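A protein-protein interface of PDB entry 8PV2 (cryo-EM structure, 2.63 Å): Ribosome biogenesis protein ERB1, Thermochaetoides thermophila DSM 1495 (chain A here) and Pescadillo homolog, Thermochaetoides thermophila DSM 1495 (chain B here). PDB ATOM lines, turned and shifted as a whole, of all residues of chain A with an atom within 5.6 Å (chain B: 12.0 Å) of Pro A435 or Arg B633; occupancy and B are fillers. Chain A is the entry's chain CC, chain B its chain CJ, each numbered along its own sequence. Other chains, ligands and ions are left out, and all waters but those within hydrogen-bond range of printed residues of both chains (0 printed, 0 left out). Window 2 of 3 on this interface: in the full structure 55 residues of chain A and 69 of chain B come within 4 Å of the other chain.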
ATOM      1  N   LEU A 432      -1.315  15.403  13.405  1.00  0.00           N
ATOM      2  CA  LEU A 432      -1.816  16.255  14.462  1.00  0.00           C
ATOM      3  C   LEU A 432      -1.722  17.712  14.039  1.00  0.00           C
ATOM      4  O   LEU A 432      -0.705  18.119  13.460  1.00  0.00           O
ATOM      5  CB  LEU A 432      -1.022  16.040  15.756  1.00  0.00           C
ATOM      6  CG  LEU A 432      -1.077  14.645  16.371  1.00  0.00           C
ATOM      7  CD1 LEU A 432       0.028  14.489  17.388  1.00  0.00           C
ATOM      8  CD2 LEU A 432      -2.430  14.402  17.005  1.00  0.00           C
ATOM      9  N   PRO A 433      -2.754  18.517  14.285  1.00  0.00           N
ATOM     10  CA  PRO A 433      -2.648  19.954  14.023  1.00  0.00           C
ATOM     11  C   PRO A 433      -1.607  20.601  14.920  1.00  0.00           C
ATOM     12  O   PRO A 433      -1.346  20.145  16.034  1.00  0.00           O
ATOM     13  CB  PRO A 433      -4.054  20.474  14.335  1.00  0.00           C
ATOM     14  CG  PRO A 433      -4.935  19.291  14.160  1.00  0.00           C
ATOM     15  CD  PRO A 433      -4.129  18.119  14.619  1.00  0.00           C
ATOM     16  N   SER A 434      -0.998  21.665  14.409  1.00  0.00           N
ATOM     17  CA  SER A 434       0.012  22.376  15.169  1.00  0.00           C
ATOM     18  C   SER A 434      -0.634  23.092  16.354  1.00  0.00           C
ATOM     19  O   SER A 434      -1.770  23.566  16.257  1.00  0.00           O
ATOM     20  CB  SER A 434       0.739  23.379  14.276  1.00  0.00           C
ATOM     21  OG  SER A 434       1.575  24.231  15.038  1.00  0.00           O
ATOM     22  N   PRO A 435       0.064  23.170  17.494  1.00  0.00           N
ATOM     23  CA  PRO A 435      -0.512  23.870  18.658  1.00  0.00           C
ATOM     24  C   PRO A 435      -0.704  25.362  18.445  1.00  0.00           C
ATOM     25  O   PRO A 435      -1.452  26.004  19.197  1.00  0.00           O
ATOM     26  CB  PRO A 435       0.503  23.580  19.773  1.00  0.00           C
ATOM     27  CG  PRO A 435       1.754  23.186  19.072  1.00  0.00           C
ATOM     28  CD  PRO A 435       1.327  22.495  17.825  1.00  0.00           C
ATOM     29  N   ASP A 436      -0.031  25.937  17.445  1.00  0.00           N
ATOM     30  CA  ASP A 436      -0.218  27.348  17.130  1.00  0.00           C
ATOM     31  C   ASP A 436      -1.634  27.622  16.640  1.00  0.00           C
ATOM     32  O   ASP A 436      -2.168  28.719  16.839  1.00  0.00           O
ATOM     33  CB  ASP A 436       0.807  27.785  16.087  1.00  0.00           C
ATOM     34  CG  ASP A 436       2.226  27.715  16.607  1.00  0.00           C
ATOM     35  OD1 ASP A 436       2.415  27.851  17.834  1.00  0.00           O
ATOM     36  OD2 ASP A 436       3.151  27.518  15.792  1.00  0.00           O
ATOM     37  N   GLU A 437      -2.256  26.638  15.990  1.00  0.00           N
ATOM     38  CA  GLU A 437      -3.662  26.774  15.628  1.00  0.00           C
ATOM     39  C   GLU A 437      -4.567  26.623  16.842  1.00  0.00           C
ATOM     40  O   GLU A 437      -5.683  27.155  16.853  1.00  0.00           O
ATOM     41  CB  GLU A 437      -4.038  25.742  14.567  1.00  0.00           C
ATOM     42  CG  GLU A 437      -2.986  25.530  13.497  1.00  0.00           C
ATOM     43  CD  GLU A 437      -3.321  24.367  12.585  1.00  0.00           C
ATOM     44  OE1 GLU A 437      -2.643  24.203  11.550  1.00  0.00           O
ATOM     45  OE2 GLU A 437      -4.264  23.615  12.906  1.00  0.00           O
ATOM     46  N   LEU A 438      -4.112  25.905  17.866  1.00  0.00           N
ATOM     47  CA  LEU A 438      -4.941  25.558  19.010  1.00  0.00           C
ATOM     48  C   LEU A 438      -4.654  26.404  20.244  1.00  0.00           C
ATOM     49  O   LEU A 438      -5.166  26.088  21.323  1.00  0.00           O
ATOM     50  CB  LEU A 438      -4.769  24.078  19.341  1.00  0.00           C
ATOM     51  CG  LEU A 438      -4.835  23.175  18.113  1.00  0.00           C
ATOM     52  CD1 LEU A 438      -4.249  21.823  18.428  1.00  0.00           C
ATOM     53  CD2 LEU A 438      -6.263  23.040  17.624  1.00  0.00           C
ATOM     54  N   LYS A 439      -3.845  27.451  20.118  1.00  0.00           N
ATOM     55  CA  LYS A 439      -3.658  28.376  21.228  1.00  0.00           C
ATOM     56  C   LYS A 439      -4.960  29.131  21.503  1.00  0.00           C
ATOM     57  O   LYS A 439      -5.789  29.279  20.600  1.00  0.00           O
ATOM     58  CB  LYS A 439      -2.520  29.353  20.920  1.00  0.00           C
ATOM     59  CG  LYS A 439      -2.787  30.307  19.779  1.00  0.00           C
ATOM     60  CD  LYS A 439      -1.700  31.361  19.703  1.00  0.00           C
ATOM     61  CE  LYS A 439      -0.385  30.763  19.241  1.00  0.00           C
ATOM     62  NZ  LYS A 439       0.658  31.807  19.054  1.00  0.00           N
ATOM     63  N   PHE A 441      -3.195  28.293  25.525  1.00  0.00           N
ATOM     64  CA  PHE A 441      -2.974  27.259  26.522  1.00  0.00           C
ATOM     65  C   PHE A 441      -1.853  27.721  27.440  1.00  0.00           C
ATOM     66  O   PHE A 441      -1.018  28.535  27.029  1.00  0.00           O
ATOM     67  CB  PHE A 441      -2.622  25.906  25.879  1.00  0.00           C
ATOM     68  CG  PHE A 441      -1.590  25.988  24.790  1.00  0.00           C
ATOM     69  CD1 PHE A 441      -1.975  26.093  23.467  1.00  0.00           C
ATOM     70  CD2 PHE A 441      -0.239  25.943  25.088  1.00  0.00           C
ATOM     71  CE1 PHE A 441      -1.037  26.164  22.465  1.00  0.00           C
ATOM     72  CE2 PHE A 441       0.703  26.013  24.086  1.00  0.00           C
ATOM     73  CZ  PHE A 441       0.303  26.125  22.775  1.00  0.00           C
ATOM     74  N   PHE A 715       2.020   9.805  27.108  1.00  0.00           N
ATOM     75  CA  PHE A 715       2.968  10.893  26.931  1.00  0.00           C
ATOM     76  C   PHE A 715       3.945  11.040  28.087  1.00  0.00           C
ATOM     77  O   PHE A 715       4.812  11.917  28.032  1.00  0.00           O
ATOM     78  CB  PHE A 715       2.222  12.214  26.736  1.00  0.00           C
ATOM     79  CG  PHE A 715       1.510  12.317  25.426  1.00  0.00           C
ATOM     80  CD1 PHE A 715       0.222  11.838  25.286  1.00  0.00           C
ATOM     81  CD2 PHE A 715       2.128  12.889  24.334  1.00  0.00           C
ATOM     82  CE1 PHE A 715      -0.435  11.930  24.083  1.00  0.00           C
ATOM     83  CE2 PHE A 715       1.476  12.984  23.129  1.00  0.00           C
ATOM     84  CZ  PHE A 715       0.192  12.505  23.006  1.00  0.00           C
ATOM     85  N   VAL A 760      -5.685  16.712  20.778  1.00  0.00           N
ATOM     86  CA  VAL A 760      -4.341  17.021  20.282  1.00  0.00           C
ATOM     87  C   VAL A 760      -3.461  17.464  21.447  1.00  0.00           C
ATOM     88  O   VAL A 760      -3.857  18.353  22.207  1.00  0.00           O
ATOM     89  CB  VAL A 760      -4.369  18.121  19.204  1.00  0.00           C
ATOM     90  CG1 VAL A 760      -2.965  18.385  18.684  1.00  0.00           C
ATOM     91  CG2 VAL A 760      -5.307  17.775  18.065  1.00  0.00           C
ATOM     92  N   PRO A 761      -2.269  16.900  21.629  1.00  0.00           N
ATOM     93  CA  PRO A 761      -1.344  17.457  22.625  1.00  0.00           C
ATOM     94  C   PRO A 761      -0.813  18.810  22.186  1.00  0.00           C
ATOM     95  O   PRO A 761      -0.363  18.973  21.051  1.00  0.00           O
ATOM     96  CB  PRO A 761      -0.225  16.413  22.691  1.00  0.00           C
ATOM     97  CG  PRO A 761      -0.307  15.691  21.398  1.00  0.00           C
ATOM     98  CD  PRO A 761      -1.752  15.665  21.021  1.00  0.00           C
ATOM     99  N   VAL A 762      -0.870  19.796  23.083  1.00  0.00           N
ATOM    100  CA  VAL A 762      -0.429  21.149  22.766  1.00  0.00           C
ATOM    101  C   VAL A 762       0.809  21.551  23.567  1.00  0.00           C
ATOM    102  O   VAL A 762       1.668  22.271  23.060  1.00  0.00           O
ATOM    103  CB  VAL A 762      -1.570  22.180  22.929  1.00  0.00           C
ATOM    104  CG1 VAL A 762      -2.589  22.007  21.825  1.00  0.00           C
ATOM    105  CG2 VAL A 762      -2.238  22.085  24.271  1.00  0.00           C
ATOM    106  N   LYS B 624      15.871  19.890  13.750  1.00  0.00           N
ATOM    107  CA  LYS B 624      15.843  18.518  14.251  1.00  0.00           C
ATOM    108  C   LYS B 624      15.081  18.418  15.567  1.00  0.00           C
ATOM    109  O   LYS B 624      14.371  17.435  15.803  1.00  0.00           O
ATOM    110  CB  LYS B 624      17.262  17.975  14.414  1.00  0.00           C
ATOM    111  CG  LYS B 624      18.007  17.786  13.108  1.00  0.00           C
ATOM    112  CD  LYS B 624      19.383  17.194  13.345  1.00  0.00           C
ATOM    113  CE  LYS B 624      20.161  17.079  12.046  1.00  0.00           C
ATOM    114  NZ  LYS B 624      19.561  16.071  11.129  1.00  0.00           N
ATOM    115  N   LYS B 625      15.216  19.423  16.437  1.00  0.00           N
ATOM    116  CA  LYS B 625      14.454  19.421  17.685  1.00  0.00           C
ATOM    117  C   LYS B 625      12.955  19.535  17.429  1.00  0.00           C
ATOM    118  O   LYS B 625      12.152  18.867  18.093  1.00  0.00           O
ATOM    119  CB  LYS B 625      14.928  20.547  18.602  1.00  0.00           C
ATOM    120  CG  LYS B 625      16.339  20.362  19.124  1.00  0.00           C
ATOM    121  CD  LYS B 625      16.731  21.481  20.070  1.00  0.00           C
ATOM    122  CE  LYS B 625      18.172  21.332  20.523  1.00  0.00           C
ATOM    123  NZ  LYS B 625      18.357  20.133  21.386  1.00  0.00           N
ATOM    124  N   GLN B 626      12.558  20.375  16.468  1.00  0.00           N
ATOM    125  CA  GLN B 626      11.144  20.482  16.112  1.00  0.00           C
ATOM    126  C   GLN B 626      10.606  19.169  15.552  1.00  0.00           C
ATOM    127  O   GLN B 626       9.495  18.738  15.903  1.00  0.00           O
ATOM    128  CB  GLN B 626      10.945  21.615  15.106  1.00  0.00           C
ATOM    129  CG  GLN B 626       9.502  21.839  14.699  1.00  0.00           C
ATOM    130  CD  GLN B 626       8.624  22.237  15.865  1.00  0.00           C
ATOM    131  OE1 GLN B 626       7.842  21.433  16.370  1.00  0.00           O
ATOM    132  NE2 GLN B 626       8.747  23.486  16.300  1.00  0.00           N
ATOM    133  N   GLU B 627      11.386  18.515  14.686  1.00  0.00           N
ATOM    134  CA  GLU B 627      10.963  17.232  14.131  1.00  0.00           C
ATOM    135  C   GLU B 627      10.862  16.166  15.214  1.00  0.00           C
ATOM    136  O   GLU B 627       9.937  15.343  15.201  1.00  0.00           O
ATOM    137  CB  GLU B 627      11.925  16.794  13.031  1.00  0.00           C
ATOM    138  CG  GLU B 627      11.884  17.677  11.796  1.00  0.00           C
ATOM    139  CD  GLU B 627      10.566  17.586  11.053  1.00  0.00           C
ATOM    140  OE1 GLU B 627       9.954  16.496  11.052  1.00  0.00           O
ATOM    141  OE2 GLU B 627      10.140  18.605  10.474  1.00  0.00           O
ATOM    142  N   ALA B 628      11.798  16.172  16.167  1.00  0.00           N
ATOM    143  CA  ALA B 628      11.747  15.224  17.275  1.00  0.00           C
ATOM    144  C   ALA B 628      10.530  15.465  18.159  1.00  0.00           C
ATOM    145  O   ALA B 628       9.915  14.511  18.646  1.00  0.00           O
ATOM    146  CB  ALA B 628      13.032  15.310  18.095  1.00  0.00           C
ATOM    147  N   GLU B 629      10.171  16.733  18.379  1.00  0.00           N
ATOM    148  CA  GLU B 629       8.985  17.039  19.174  1.00  0.00           C
ATOM    149  C   GLU B 629       7.711  16.557  18.487  1.00  0.00           C
ATOM    150  O   GLU B 629       6.822  15.983  19.135  1.00  0.00           O
ATOM    151  CB  GLU B 629       8.912  18.541  19.447  1.00  0.00           C
ATOM    152  CG  GLU B 629       7.753  18.955  20.335  1.00  0.00           C
ATOM    153  CD  GLU B 629       7.899  18.457  21.760  1.00  0.00           C
ATOM    154  OE1 GLU B 629       9.048  18.304  22.227  1.00  0.00           O
ATOM    155  OE2 GLU B 629       6.863  18.216  22.415  1.00  0.00           O
ATOM    156  N   GLU B 630       7.608  16.774  17.171  1.00  0.00           N
ATOM    157  CA  GLU B 630       6.453  16.270  16.428  1.00  0.00           C
ATOM    158  C   GLU B 630       6.396  14.744  16.452  1.00  0.00           C
ATOM    159  O   GLU B 630       5.312  14.151  16.587  1.00  0.00           O
ATOM    160  CB  GLU B 630       6.494  16.783  14.991  1.00  0.00           C
ATOM    161  CG  GLU B 630       5.209  16.558  14.218  1.00  0.00           C
ATOM    162  CD  GLU B 630       3.977  16.989  14.988  1.00  0.00           C
ATOM    163  OE1 GLU B 630       3.924  18.155  15.434  1.00  0.00           O
ATOM    164  OE2 GLU B 630       3.061  16.156  15.149  1.00  0.00           O
ATOM    165  N   LEU B 631       7.558  14.095  16.341  1.00  0.00           N
ATOM    166  CA  LEU B 631       7.625  12.641  16.432  1.00  0.00           C
ATOM    167  C   LEU B 631       7.176  12.146  17.800  1.00  0.00           C
ATOM    168  O   LEU B 631       6.488  11.125  17.901  1.00  0.00           O
ATOM    169  CB  LEU B 631       9.049  12.173  16.138  1.00  0.00           C
ATOM    170  CG  LEU B 631       9.313  10.671  16.193  1.00  0.00           C
ATOM    171  CD1 LEU B 631       8.524   9.965  15.118  1.00  0.00           C
ATOM    172  CD2 LEU B 631      10.797  10.385  16.050  1.00  0.00           C
ATOM    173  N   GLU B 632       7.557  12.856  18.864  1.00  0.00           N
ATOM    174  CA  GLU B 632       7.148  12.457  20.208  1.00  0.00           C
ATOM    175  C   GLU B 632       5.645  12.613  20.404  1.00  0.00           C
ATOM    176  O   GLU B 632       5.012  11.780  21.063  1.00  0.00           O
ATOM    177  CB  GLU B 632       7.911  13.264  21.256  1.00  0.00           C
ATOM    178  CG  GLU B 632       9.364  12.852  21.412  1.00  0.00           C
ATOM    179  CD  GLU B 632       9.519  11.447  21.958  1.00  0.00           C
ATOM    180  OE1 GLU B 632       8.683  11.031  22.787  1.00  0.00           O
ATOM    181  OE2 GLU B 632      10.479  10.756  21.558  1.00  0.00           O
ATOM    182  N   ARG B 633       5.058  13.673  19.842  1.00  0.00           N
ATOM    183  CA  ARG B 633       3.605  13.828  19.920  1.00  0.00           C
ATOM    184  C   ARG B 633       2.880  12.697  19.191  1.00  0.00           C
ATOM    185  O   ARG B 633       1.898  12.140  19.707  1.00  0.00           O
ATOM    186  CB  ARG B 633       3.187  15.185  19.360  1.00  0.00           C
ATOM    187  CG  ARG B 633       3.734  16.364  20.136  1.00  0.00           C
ATOM    188  CD  ARG B 633       2.882  17.603  19.935  1.00  0.00           C
ATOM    189  NE  ARG B 633       2.628  17.877  18.527  1.00  0.00           N
ATOM    190  CZ  ARG B 633       1.595  18.574  18.077  1.00  0.00           C
ATOM    191  NH1 ARG B 633       0.680  19.060  18.896  1.00  0.00           N
ATOM    192  NH2 ARG B 633       1.475  18.786  16.770  1.00  0.00           N
ATOM    193  N   ALA B 634       3.363  12.327  18.000  1.00  0.00           N
ATOM    194  CA  ALA B 634       2.741  11.221  17.270  1.00  0.00           C
ATOM    195  C   ALA B 634       2.918   9.889  18.002  1.00  0.00           C
ATOM    196  O   ALA B 634       1.995   9.062  18.042  1.00  0.00           O
ATOM    197  CB  ALA B 634       3.316  11.144  15.860  1.00  0.00           C
ATOM    198  N   LYS B 635       4.098   9.673  18.592  1.00  0.00           N
ATOM    199  CA  LYS B 635       4.346   8.471  19.385  1.00  0.00           C
ATOM    200  C   LYS B 635       3.409   8.392  20.577  1.00  0.00           C
ATOM    201  O   LYS B 635       2.925   7.308  20.924  1.00  0.00           O
ATOM    202  CB  LYS B 635       5.794   8.452  19.868  1.00  0.00           C
ATOM    203  CG  LYS B 635       6.719   7.541  19.107  1.00  0.00           C
ATOM    204  CD  LYS B 635       7.967   7.285  19.927  1.00  0.00           C
ATOM    205  CE  LYS B 635       8.784   6.146  19.356  1.00  0.00           C
ATOM    206  NZ  LYS B 635       9.983   5.854  20.188  1.00  0.00           N
ATOM    207  N   GLY B 636       3.163   9.525  21.233  1.00  0.00           N
ATOM    208  CA  GLY B 636       2.214   9.537  22.330  1.00  0.00           C
ATOM    209  C   GLY B 636       0.801   9.229  21.881  1.00  0.00           C
ATOM    210  O   GLY B 636       0.047   8.556  22.586  1.00  0.00           O
ATOM    211  N   MET B 637       0.423   9.710  20.695  1.00  0.00           N
ATOM    212  CA  MET B 637      -0.929   9.449  20.208  1.00  0.00           C
ATOM    213  C   MET B 637      -1.101   8.005  19.752  1.00  0.00           C
ATOM    214  O   MET B 637      -2.231   7.513  19.655  1.00  0.00           O
ATOM    215  CB  MET B 637      -1.273  10.413  19.077  1.00  0.00           C
ATOM    216  CG  MET B 637      -1.610  11.808  19.554  1.00  0.00           C
ATOM    217  SD  MET B 637      -2.697  11.792  20.987  1.00  0.00           S
ATOM    218  CE  MET B 637      -4.297  11.766  20.190  1.00  0.00           C
ATOM    219  N   LEU B 638       0.000   7.315  19.450  1.00  0.00           N
ATOM    220  CA  LEU B 638      -0.087   5.910  19.048  1.00  0.00           C
ATOM    221  C   LEU B 638      -0.607   5.015  20.170  1.00  0.00           C
ATOM    222  O   LEU B 638      -0.415   5.285  21.356  1.00  0.00           O
ATOM    223  CB  LEU B 638       1.275   5.386  18.603  1.00  0.00           C
ATOM    224  CG  LEU B 638       1.729   5.665  17.180  1.00  0.00           C
ATOM    225  CD1 LEU B 638       3.037   4.947  16.934  1.00  0.00           C
ATOM    226  CD2 LEU B 638       0.667   5.201  16.210  1.00  0.00           C
ATOM    227  N   SER B 639      -1.264   3.925  19.772  1.00  0.00           N
ATOM    228  CA  SER B 639      -1.685   2.896  20.713  1.00  0.00           C
ATOM    229  C   SER B 639      -0.524   1.959  21.027  1.00  0.00           C
ATOM    230  O   SER B 639       0.522   1.993  20.380  1.00  0.00           O
ATOM    231  CB  SER B 639      -2.862   2.096  20.160  1.00  0.00           C
ATOM    232  OG  SER B 639      -2.408   1.025  19.356  1.00  0.00           O
ATOM    233  N   LYS B 640      -0.745   1.086  22.014  1.00  0.00           N
ATOM    234  CA  LYS B 640       0.355   0.407  22.698  1.00  0.00           C
ATOM    235  C   LYS B 640       1.095  -0.572  21.789  1.00  0.00           C
ATOM    236  O   LYS B 640       2.329  -0.519  21.678  1.00  0.00           O
ATOM    237  CB  LYS B 640      -0.195  -0.308  23.931  1.00  0.00           C
ATOM    238  CG  LYS B 640       0.845  -0.856  24.874  1.00  0.00           C
ATOM    239  CD  LYS B 640       0.171  -1.453  26.086  1.00  0.00           C
ATOM    240  CE  LYS B 640       1.170  -2.060  27.043  1.00  0.00           C
ATOM    241  NZ  LYS B 640       0.481  -2.640  28.223  1.00  0.00           N
ATOM    242  N   LYS B 642       0.848  -0.747  18.481  1.00  0.00           N
ATOM    243  CA  LYS B 642       1.373   0.052  17.380  1.00  0.00           C
ATOM    244  C   LYS B 642       2.612   0.828  17.803  1.00  0.00           C
ATOM    245  O   LYS B 642       3.544   0.989  17.011  1.00  0.00           O
ATOM    246  CB  LYS B 642       0.300   1.002  16.854  1.00  0.00           C
ATOM    247  CG  LYS B 642      -0.994   0.334  16.420  1.00  0.00           C
ATOM    248  CD  LYS B 642      -0.824  -0.489  15.149  1.00  0.00           C
ATOM    249  CE  LYS B 642      -0.926  -1.984  15.425  1.00  0.00           C
ATOM    250  NZ  LYS B 642      -0.896  -2.780  14.169  1.00  0.00           N
ATOM    251  N   ARG B 643       2.642   1.309  19.051  1.00  0.00           N
ATOM    252  CA  ARG B 643       3.840   1.963  19.570  1.00  0.00           C
ATOM    253  C   ARG B 643       5.022   1.011  19.602  1.00  0.00           C
ATOM    254  O   ARG B 643       6.144   1.393  19.249  1.00  0.00           O
ATOM    255  CB  ARG B 643       3.588   2.510  20.975  1.00  0.00           C
ATOM    256  CG  ARG B 643       4.104   3.910  21.220  1.00  0.00           C
ATOM    257  CD  ARG B 643       3.673   4.397  22.589  1.00  0.00           C
ATOM    258  NE  ARG B 643       4.204   5.717  22.900  1.00  0.00           N
ATOM    259  CZ  ARG B 643       5.364   5.935  23.503  1.00  0.00           C
ATOM    260  NH1 ARG B 643       6.154   4.936  23.857  1.00  0.00           N
ATOM    261  NH2 ARG B 643       5.740   7.185  23.755  1.00  0.00           N
ATOM    262  N   PHE B 646       6.211   0.402  16.086  1.00  0.00           N
ATOM    263  CA  PHE B 646       6.869   1.605  15.593  1.00  0.00           C
ATOM    264  C   PHE B 646       8.270   1.745  16.169  1.00  0.00           C
ATOM    265  O   PHE B 646       9.211   2.111  15.453  1.00  0.00           O
ATOM    266  CB  PHE B 646       6.018   2.825  15.936  1.00  0.00           C
ATOM    267  CG  PHE B 646       6.584   4.120  15.449  1.00  0.00           C
ATOM    268  CD1 PHE B 646       6.530   4.452  14.110  1.00  0.00           C
ATOM    269  CD2 PHE B 646       7.168   5.007  16.331  1.00  0.00           C
ATOM    270  CE1 PHE B 646       7.049   5.643  13.662  1.00  0.00           C
ATOM    271  CE2 PHE B 646       7.689   6.199  15.884  1.00  0.00           C
ATOM    272  CZ  PHE B 646       7.630   6.516  14.549  1.00  0.00           C
ATOM    273  N   GLU B 647       8.432   1.445  17.460  1.00  0.00           N
ATOM    274  CA  GLU B 647       9.754   1.495  18.071  1.00  0.00           C
ATOM    275  C   GLU B 647      10.680   0.440  17.483  1.00  0.00           C
ATOM    276  O   GLU B 647      11.879   0.689  17.314  1.00  0.00           O
ATOM    277  CB  GLU B 647       9.651   1.328  19.585  1.00  0.00           C
ATOM    278  CG  GLU B 647       9.103   2.542  20.303  1.00  0.00           C
ATOM    279  CD  GLU B 647       8.336   2.180  21.554  1.00  0.00           C
ATOM    280  OE1 GLU B 647       8.408   1.005  21.974  1.00  0.00           O
ATOM    281  OE2 GLU B 647       7.662   3.066  22.117  1.00  0.00           O
ATOM    282  N   GLN B 650      11.808   1.767  14.133  1.00  0.00           N
ATOM    283  CA  GLN B 650      12.778   2.836  14.341  1.00  0.00           C
ATOM    284  C   GLN B 650      14.133   2.286  14.760  1.00  0.00           C
ATOM    285  O   GLN B 650      15.170   2.794  14.328  1.00  0.00           O
ATOM    286  CB  GLN B 650      12.261   3.819  15.386  1.00  0.00           C
ATOM    287  CG  GLN B 650      11.227   4.784  14.859  1.00  0.00           C
ATOM    288  CD  GLN B 650      11.097   6.006  15.732  1.00  0.00           C
ATOM    289  OE1 GLN B 650      10.860   7.109  15.243  1.00  0.00           O
ATOM    290  NE2 GLN B 650      11.261   5.821  17.035  1.00  0.00           N
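Among the printed residues, merely in contact across the chains: Leu A432 with Arg B633 (3.8 Å), Leu A432 with Met B637 (3.7 Å), Pro A435 with Arg B633 (3.7 Å), Phe A715 with Arg B633 (3.5 Å), Phe A715 with Gly B636 (3.5 Å), Phe A715 with Met B637 (3.6 Å), Val A760 with Arg B633 (3.7 Å) and Pro A761 with Met B637 (3.99 Å).
The side-chain carboxylate (OE1) of Glu B630 lies within salt-bridge range of the guanidinium group (NH2) of Arg B633 (2.9 Å).
Leu A432 touches just these residues of chain B: Arg B633 and Met B637. Of chain B, only Arg B633 (3.2 Å) comes within 4 Å of Pro A433. No residue of chain B comes within 4 Å of Ser A434. No residue of chain B comes within 4 Å of Asp A436. No residue of chain B comes within 4 Å of Glu A437. No residue of chain B comes within 4 Å of Leu A438. No residue of chain B comes within 4 Å of Lys A439. Printed residues of chain B within 4 Å of Phe A715: Arg B633 (3.5 Å), Gly B636 (3.5 Å) and Met B637 (3.6 Å). Val A760 touches just one residue of chain B: Arg B633 (3.7 Å). Of the printed residues of chain B, Pro A761 touches Arg B633 (2.4 Å) and Met B637 (3.99 Å). Gln B626 touches none of the printed residues of chain A. Arg B633 touches six residues of chain A. Of the printed residues of chain A, Met B637 touches Leu A432 (3.7 Å), Phe A715 (3.6 Å) and Pro A761 (3.99 Å). Arg B643 touches none of the printed residues of chain A. The nearest printed residue of chain A that does not touch Gly B636 is Pro A761 (6.6 Å).
Along chain B the printed residues that touch a printed residue of chain A span positions 633 to 637. Hydrophobic or aromatic side chains of chain A within 4 Å of the printed part of chain B: Leu A432, Pro A435, Phe A715, Val A760 and Pro A761.
O of Pro A433 sits at hydrogen-bond distance from NH2 of Arg B633. The backbone carbonyl oxygen (O) of Pro A761 sits close to the guanidinium group (NH1) of Arg B633, 2.4 Å away.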
